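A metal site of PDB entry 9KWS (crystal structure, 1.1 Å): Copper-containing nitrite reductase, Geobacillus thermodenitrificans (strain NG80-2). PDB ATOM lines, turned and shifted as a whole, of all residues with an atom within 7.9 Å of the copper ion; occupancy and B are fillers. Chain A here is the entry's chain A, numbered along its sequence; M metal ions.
The backbone carbonyl oxygen (O) of His 95 lies within hydrogen-bond range of the backbone NH (N) of Val 113, at 2.7 Å.
A ring nitrogen (NE2) of His 95 sits close to the backbone carbonyl oxygen (O) of Val 93 (3.4 Å).
OG1 of Thr 137 lies close to SG of Cys 135 (3.4 Å).
The backbone NH (N) of Met 148 sits close to the backbone carbonyl oxygen (O) of Trp 63.
N of Ser 96 lies close to SG of Cys 135, 3.4 Å away.
A ring nitrogen (NE2) of His 95 sits at hydrogen-bond distance from the side-chain carboxylate of Asp 90 (2.8 Å).
The copper ion is bound by a ring nitrogen (ND1) of His 95 (2.0 Å), a ring nitrogen (ND1) of His 143 (2.1 Å), the side-chain sulfur (SG) of Cys 135 (2.2 Å) and the side-chain sulfur (SD) of Met 148 (2.6 Å).
The copper ion has four donor atoms within binding distance.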
ATOM      1  N   ALA A  47      -9.079 -22.583  13.268  1.00  0.00           N
ATOM      2  CA  ALA A  47      -8.204 -23.546  13.938  1.00  0.00           C
ATOM      3  C   ALA A  47      -8.663 -23.597  15.384  1.00  0.00           C
ATOM      4  O   ALA A  47      -8.801 -22.548  16.015  1.00  0.00           O
ATOM      5  CB  ALA A  47      -6.742 -23.123  13.864  1.00  0.00           C
ATOM      6  N   TRP A  63      -6.050 -31.039  17.551  1.00  0.00           N
ATOM      7  CA  TRP A  63      -5.856 -29.763  16.871  1.00  0.00           C
ATOM      8  C   TRP A  63      -6.593 -29.879  15.554  1.00  0.00           C
ATOM      9  O   TRP A  63      -6.353 -30.833  14.800  1.00  0.00           O
ATOM     10  CB  TRP A  63      -4.380 -29.500  16.637  1.00  0.00           C
ATOM     11  CG  TRP A  63      -3.491 -29.466  17.849  1.00  0.00           C
ATOM     12  CD1 TRP A  63      -3.795 -29.748  19.142  1.00  0.00           C
ATOM     13  CD2 TRP A  63      -2.112 -29.105  17.844  1.00  0.00           C
ATOM     14  NE1 TRP A  63      -2.685 -29.593  19.942  1.00  0.00           N
ATOM     15  CE2 TRP A  63      -1.636 -29.192  19.156  1.00  0.00           C
ATOM     16  CE3 TRP A  63      -1.222 -28.728  16.827  1.00  0.00           C
ATOM     17  CZ2 TRP A  63      -0.311 -28.908  19.495  1.00  0.00           C
ATOM     18  CZ3 TRP A  63       0.088 -28.472  17.167  1.00  0.00           C
ATOM     19  CH2 TRP A  63       0.535 -28.554  18.489  1.00  0.00           C
ATOM     20  N   THR A  64      -7.526 -28.958  15.289  1.00  0.00           N
ATOM     21  CA  THR A  64      -8.458 -29.170  14.198  1.00  0.00           C
ATOM     22  C   THR A  64      -8.712 -27.902  13.404  1.00  0.00           C
ATOM     23  O   THR A  64      -8.524 -26.782  13.891  1.00  0.00           O
ATOM     24  CB  THR A  64      -9.844 -29.653  14.673  1.00  0.00           C
ATOM     25  OG1 THR A  64     -10.575 -28.570  15.277  1.00  0.00           O
ATOM     26  CG2 THR A  64      -9.734 -30.818  15.648  1.00  0.00           C
ATOM     27  N   PHE A  65      -9.221 -28.108  12.201  1.00  0.00           N
ATOM     28  CA  PHE A  65      -9.994 -27.101  11.495  1.00  0.00           C
ATOM     29  C   PHE A  65     -11.470 -27.312  11.823  1.00  0.00           C
ATOM     30  O   PHE A  65     -12.019 -28.394  11.576  1.00  0.00           O
ATOM     31  CB  PHE A  65      -9.753 -27.193   9.986  1.00  0.00           C
ATOM     32  CG  PHE A  65      -8.331 -26.901   9.584  1.00  0.00           C
ATOM     33  CD1 PHE A  65      -7.827 -25.603   9.628  1.00  0.00           C
ATOM     34  CD2 PHE A  65      -7.479 -27.930   9.206  1.00  0.00           C
ATOM     35  CE1 PHE A  65      -6.532 -25.348   9.248  1.00  0.00           C
ATOM     36  CE2 PHE A  65      -6.174 -27.656   8.816  1.00  0.00           C
ATOM     37  CZ  PHE A  65      -5.702 -26.370   8.836  1.00  0.00           C
ATOM     38  N   LEU A  86      -8.411 -17.904   7.741  1.00  0.00           N
ATOM     39  CA  LEU A  86      -8.252 -18.752   8.915  1.00  0.00           C
ATOM     40  C   LEU A  86      -8.378 -17.884  10.160  1.00  0.00           C
ATOM     41  O   LEU A  86      -7.631 -16.917  10.324  1.00  0.00           O
ATOM     42  CB  LEU A  86      -6.888 -19.447   8.922  1.00  0.00           C
ATOM     43  CG  LEU A  86      -6.680 -20.445  10.065  1.00  0.00           C
ATOM     44  CD1 LEU A  86      -7.661 -21.611  10.004  1.00  0.00           C
ATOM     45  CD2 LEU A  86      -5.241 -20.968  10.046  1.00  0.00           C
ATOM     46  N   ASN A  88      -7.813 -18.182  14.014  1.00  0.00           N
ATOM     47  CA  ASN A  88      -7.120 -19.053  14.949  1.00  0.00           C
ATOM     48  C   ASN A  88      -7.712 -18.885  16.338  1.00  0.00           C
ATOM     49  O   ASN A  88      -7.484 -17.863  16.986  1.00  0.00           O
ATOM     50  CB  ASN A  88      -5.618 -18.800  14.950  1.00  0.00           C
ATOM     51  CG  ASN A  88      -4.887 -19.813  15.785  1.00  0.00           C
ATOM     52  OD1 ASN A  88      -5.501 -20.721  16.344  1.00  0.00           O
ATOM     53  ND2 ASN A  88      -3.574 -19.682  15.857  1.00  0.00           N
ATOM     54  N   ASP A  90      -7.045 -21.174  18.748  1.00  0.00           N
ATOM     55  CA  ASP A  90      -6.143 -21.803  19.702  1.00  0.00           C
ATOM     56  C   ASP A  90      -5.579 -20.714  20.606  1.00  0.00           C
ATOM     57  O   ASP A  90      -5.116 -19.678  20.106  1.00  0.00           O
ATOM     58  CB  ASP A  90      -5.022 -22.474  18.908  1.00  0.00           C
ATOM     59  CG  ASP A  90      -4.093 -23.354  19.756  1.00  0.00           C
ATOM     60  OD1 ASP A  90      -3.705 -22.930  20.876  1.00  0.00           O
ATOM     61  OD2 ASP A  90      -3.696 -24.442  19.269  1.00  0.00           O
ATOM     62  N   VAL A  93      -1.059 -21.701  20.299  1.00  0.00           N
ATOM     63  CA  VAL A  93      -0.287 -22.233  19.172  1.00  0.00           C
ATOM     64  C   VAL A  93      -0.692 -21.527  17.882  1.00  0.00           C
ATOM     65  O   VAL A  93      -1.890 -21.461  17.584  1.00  0.00           O
ATOM     66  CB  VAL A  93      -0.445 -23.756  19.032  1.00  0.00           C
ATOM     67  CG1 VAL A  93       0.533 -24.279  18.000  1.00  0.00           C
ATOM     68  CG2 VAL A  93      -0.237 -24.465  20.342  1.00  0.00           C
ATOM     69  N   PRO A  94       0.260 -21.014  17.103  1.00  0.00           N
ATOM     70  CA  PRO A  94      -0.067 -20.532  15.748  1.00  0.00           C
ATOM     71  C   PRO A  94      -0.464 -21.686  14.833  1.00  0.00           C
ATOM     72  O   PRO A  94      -0.032 -22.813  15.021  1.00  0.00           O
ATOM     73  CB  PRO A  94       1.268 -19.906  15.272  1.00  0.00           C
ATOM     74  CG  PRO A  94       2.017 -19.634  16.548  1.00  0.00           C
ATOM     75  CD  PRO A  94       1.704 -20.869  17.359  1.00  0.00           C
ATOM     76  N   HIS A  95      -1.258 -21.360  13.814  1.00  0.00           N
ATOM     77  CA  HIS A  95      -1.687 -22.333  12.813  1.00  0.00           C
ATOM     78  C   HIS A  95      -1.719 -21.676  11.448  1.00  0.00           C
ATOM     79  O   HIS A  95      -1.652 -20.454  11.320  1.00  0.00           O
ATOM     80  CB  HIS A  95      -3.058 -22.929  13.168  1.00  0.00           C
ATOM     81  CG  HIS A  95      -3.044 -23.697  14.445  1.00  0.00           C
ATOM     82  ND1 HIS A  95      -2.397 -24.904  14.581  1.00  0.00           N
ATOM     83  CD2 HIS A  95      -3.569 -23.400  15.654  1.00  0.00           C
ATOM     84  CE1 HIS A  95      -2.526 -25.319  15.827  1.00  0.00           C
ATOM     85  NE2 HIS A  95      -3.234 -24.423  16.497  1.00  0.00           N
ATOM     86  N   SER A  96      -1.834 -22.506  10.414  1.00  0.00           N
ATOM     87  CA  SER A  96      -1.772 -22.031   9.040  1.00  0.00           C
ATOM     88  C   SER A  96      -2.555 -23.006   8.163  1.00  0.00           C
ATOM     89  O   SER A  96      -3.123 -23.988   8.641  1.00  0.00           O
ATOM     90  CB  SER A  96      -0.323 -21.931   8.563  1.00  0.00           C
ATOM     91  OG  SER A  96       0.318 -23.193   8.649  1.00  0.00           O
ATOM     92  N   MET A  97      -2.572 -22.719   6.867  1.00  0.00           N
ATOM     93  CA  MET A  97      -3.252 -23.549   5.875  1.00  0.00           C
ATOM     94  C   MET A  97      -2.435 -23.726   4.615  1.00  0.00           C
ATOM     95  O   MET A  97      -2.022 -22.739   3.995  1.00  0.00           O
ATOM     96  CB  MET A  97      -4.621 -22.980   5.518  1.00  0.00           C
ATOM     97  CG  MET A  97      -5.371 -23.767   4.460  1.00  0.00           C
ATOM     98  SD  MET A  97      -5.738 -25.455   4.815  1.00  0.00           S
ATOM     99  CE  MET A  97      -7.290 -25.192   5.740  1.00  0.00           C
ATOM    100  N   ASP A 112       1.798 -18.366   9.125  1.00  0.00           N
ATOM    101  CA  ASP A 112       1.134 -18.559  10.389  1.00  0.00           C
ATOM    102  C   ASP A 112       0.166 -17.429  10.724  1.00  0.00           C
ATOM    103  O   ASP A 112       0.408 -16.255  10.415  1.00  0.00           O
ATOM    104  CB  ASP A 112       2.165 -18.710  11.512  1.00  0.00           C
ATOM    105  CG  ASP A 112       2.971 -19.995  11.403  1.00  0.00           C
ATOM    106  OD1 ASP A 112       2.529 -20.939  10.720  1.00  0.00           O
ATOM    107  OD2 ASP A 112       4.068 -20.062  11.999  1.00  0.00           O
ATOM    108  N   VAL A 113      -0.925 -17.808  11.379  1.00  0.00           N
ATOM    109  CA  VAL A 113      -1.906 -16.918  11.975  1.00  0.00           C
ATOM    110  C   VAL A 113      -1.781 -17.117  13.476  1.00  0.00           C
ATOM    111  O   VAL A 113      -1.886 -18.248  13.972  1.00  0.00           O
ATOM    112  CB  VAL A 113      -3.315 -17.239  11.475  1.00  0.00           C
ATOM    113  CG1 VAL A 113      -4.344 -16.349  12.151  1.00  0.00           C
ATOM    114  CG2 VAL A 113      -3.384 -17.112   9.955  1.00  0.00           C
ATOM    115  N   HIS A 134      -3.890 -29.130   4.861  1.00  0.00           N
ATOM    116  CA  HIS A 134      -3.411 -29.345   6.213  1.00  0.00           C
ATOM    117  C   HIS A 134      -2.775 -28.076   6.742  1.00  0.00           C
ATOM    118  O   HIS A 134      -2.391 -27.192   5.997  1.00  0.00           O
ATOM    119  CB  HIS A 134      -2.397 -30.507   6.272  1.00  0.00           C
ATOM    120  CG  HIS A 134      -1.202 -30.311   5.393  1.00  0.00           C
ATOM    121  ND1 HIS A 134      -0.065 -29.647   5.805  1.00  0.00           N
ATOM    122  CD2 HIS A 134      -0.942 -30.720   4.121  1.00  0.00           C
ATOM    123  CE1 HIS A 134       0.836 -29.667   4.833  1.00  0.00           C
ATOM    124  NE2 HIS A 134       0.325 -30.302   3.800  1.00  0.00           N
ATOM    125  N   CYS A 135      -2.607 -28.027   8.059  1.00  0.00           N
ATOM    126  CA  CYS A 135      -1.825 -26.959   8.645  1.00  0.00           C
ATOM    127  C   CYS A 135      -0.364 -27.104   8.228  1.00  0.00           C
ATOM    128  O   CYS A 135       0.171 -28.213   8.151  1.00  0.00           O
ATOM    129  CB  CYS A 135      -1.951 -27.014  10.155  1.00  0.00           C
ATOM    130  SG  CYS A 135      -1.012 -25.720  11.017  1.00  0.00           S
ATOM    131  N   GLY A 136       0.266 -25.972   7.947  1.00  0.00           N
ATOM    132  CA  GLY A 136       1.647 -25.924   7.515  1.00  0.00           C
ATOM    133  C   GLY A 136       2.602 -25.295   8.500  1.00  0.00           C
ATOM    134  O   GLY A 136       3.669 -24.826   8.103  1.00  0.00           O
ATOM    135  N   THR A 137       2.260 -25.270   9.784  1.00  0.00           N
ATOM    136  CA  THR A 137       3.072 -24.636  10.817  1.00  0.00           C
ATOM    137  C   THR A 137       4.128 -25.617  11.309  1.00  0.00           C
ATOM    138  O   THR A 137       3.858 -26.798  11.540  1.00  0.00           O
ATOM    139  CB  THR A 137       2.161 -24.168  11.945  1.00  0.00           C
ATOM    140  OG1 THR A 137       1.226 -23.208  11.411  1.00  0.00           O
ATOM    141  CG2 THR A 137       2.925 -23.536  13.088  1.00  0.00           C
ATOM    142  N   LYS A 138       5.349 -25.109  11.486  1.00  0.00           N
ATOM    143  CA  LYS A 138       6.449 -25.970  11.922  1.00  0.00           C
ATOM    144  C   LYS A 138       6.273 -26.309  13.398  1.00  0.00           C
ATOM    145  O   LYS A 138       5.915 -25.448  14.194  1.00  0.00           O
ATOM    146  CB  LYS A 138       7.781 -25.229  11.721  1.00  0.00           C
ATOM    147  CG  LYS A 138       8.931 -25.773  12.547  1.00  0.00           C
ATOM    148  CD  LYS A 138      10.289 -25.434  11.938  1.00  0.00           C
ATOM    149  CE  LYS A 138      11.350 -26.364  12.512  1.00  0.00           C
ATOM    150  NZ  LYS A 138      10.720 -27.548  13.188  1.00  0.00           N
ATOM    151  N   PRO A 139       6.511 -27.573  13.804  1.00  0.00           N
ATOM    152  CA  PRO A 139       6.824 -28.749  12.967  1.00  0.00           C
ATOM    153  C   PRO A 139       5.552 -29.288  12.321  1.00  0.00           C
ATOM    154  O   PRO A 139       4.578 -29.601  13.003  1.00  0.00           O
ATOM    155  CB  PRO A 139       7.373 -29.772  13.964  1.00  0.00           C
ATOM    156  CG  PRO A 139       7.418 -29.112  15.278  1.00  0.00           C
ATOM    157  CD  PRO A 139       6.534 -27.918  15.237  1.00  0.00           C
ATOM    158  N   VAL A 140       5.563 -29.393  10.990  1.00  0.00           N
ATOM    159  CA  VAL A 140       4.350 -29.773  10.279  1.00  0.00           C
ATOM    160  C   VAL A 140       3.868 -31.147  10.705  1.00  0.00           C
ATOM    161  O   VAL A 140       2.668 -31.365  10.847  1.00  0.00           O
ATOM    162  CB  VAL A 140       4.579 -29.656   8.758  1.00  0.00           C
ATOM    163  CG1 VAL A 140       3.394 -30.190   7.990  1.00  0.00           C
ATOM    164  CG2 VAL A 140       4.853 -28.214   8.379  1.00  0.00           C
ATOM    165  N   GLN A 142       3.850 -32.412  13.607  1.00  0.00           N
ATOM    166  CA  GLN A 142       3.073 -32.260  14.840  1.00  0.00           C
ATOM    167  C   GLN A 142       1.663 -31.751  14.549  1.00  0.00           C
ATOM    168  O   GLN A 142       0.674 -32.244  15.119  1.00  0.00           O
ATOM    169  CB  GLN A 142       3.801 -31.302  15.785  1.00  0.00           C
ATOM    170  CG  GLN A 142       3.137 -31.155  17.130  1.00  0.00           C
ATOM    171  CD  GLN A 142       3.936 -30.294  18.078  1.00  0.00           C
ATOM    172  OE1 GLN A 142       4.801 -29.524  17.660  1.00  0.00           O
ATOM    173  NE2 GLN A 142       3.653 -30.425  19.359  1.00  0.00           N
ATOM    174  N   HIS A 143       1.553 -30.752  13.684  1.00  0.00           N
ATOM    175  CA  HIS A 143       0.238 -30.190  13.393  1.00  0.00           C
ATOM    176  C   HIS A 143      -0.637 -31.179  12.627  1.00  0.00           C
ATOM    177  O   HIS A 143      -1.829 -31.357  12.955  1.00  0.00           O
ATOM    178  CB  HIS A 143       0.415 -28.866  12.673  1.00  0.00           C
ATOM    179  CG  HIS A 143       0.945 -27.789  13.575  1.00  0.00           C
ATOM    180  ND1 HIS A 143       0.148 -26.782  14.058  1.00  0.00           N
ATOM    181  CD2 HIS A 143       2.172 -27.587  14.101  1.00  0.00           C
ATOM    182  CE1 HIS A 143       0.873 -25.989  14.827  1.00  0.00           C
ATOM    183  NE2 HIS A 143       2.098 -26.454  14.876  1.00  0.00           N
ATOM    184  N   ILE A 144      -0.062 -31.869  11.631  1.00  0.00           N
ATOM    185  CA  ILE A 144      -0.854 -32.881  10.931  1.00  0.00           C
ATOM    186  C   ILE A 144      -1.243 -33.993  11.893  1.00  0.00           C
ATOM    187  O   ILE A 144      -2.417 -34.385  11.977  1.00  0.00           O
ATOM    188  CB  ILE A 144      -0.109 -33.427   9.704  1.00  0.00           C
ATOM    189  CG1 ILE A 144       0.180 -32.329   8.675  1.00  0.00           C
ATOM    190  CG2 ILE A 144      -0.946 -34.552   9.083  1.00  0.00           C
ATOM    191  CD1 ILE A 144       0.981 -32.808   7.484  1.00  0.00           C
ATOM    192  N   ASN A 146      -1.663 -34.172  15.019  1.00  0.00           N
ATOM    193  CA  ASN A 146      -2.657 -33.818  16.026  1.00  0.00           C
ATOM    194  C   ASN A 146      -4.048 -33.580  15.458  1.00  0.00           C
ATOM    195  O   ASN A 146      -4.986 -33.399  16.247  1.00  0.00           O
ATOM    196  CB  ASN A 146      -2.202 -32.613  16.835  1.00  0.00           C
ATOM    197  CG  ASN A 146      -1.195 -32.960  17.922  1.00  0.00           C
ATOM    198  OD1 ASN A 146      -1.241 -34.033  18.526  1.00  0.00           O
ATOM    199  ND2 ASN A 146      -0.289 -32.027  18.189  1.00  0.00           N
ATOM    200  N   GLY A 147      -4.215 -33.597  14.125  1.00  0.00           N
ATOM    201  CA  GLY A 147      -5.522 -33.588  13.512  1.00  0.00           C
ATOM    202  C   GLY A 147      -5.765 -32.576  12.414  1.00  0.00           C
ATOM    203  O   GLY A 147      -6.874 -32.565  11.876  1.00  0.00           O
ATOM    204  N   MET A 148      -4.780 -31.755  12.041  1.00  0.00           N
ATOM    205  CA  MET A 148      -5.022 -30.621  11.134  1.00  0.00           C
ATOM    206  C   MET A 148      -4.783 -31.026   9.679  1.00  0.00           C
ATOM    207  O   MET A 148      -3.805 -30.647   9.039  1.00  0.00           O
ATOM    208  CB  MET A 148      -4.137 -29.440  11.526  1.00  0.00           C
ATOM    209  CG  MET A 148      -4.325 -29.055  12.983  1.00  0.00           C
ATOM    210  SD  MET A 148      -3.713 -27.447  13.462  1.00  0.00           S
ATOM    211  CE  MET A 148      -4.962 -26.431  12.739  1.00  0.00           C
HETATM  212 CU    CU M   1      -1.530 -26.036  13.128  1.00  0.00          CU
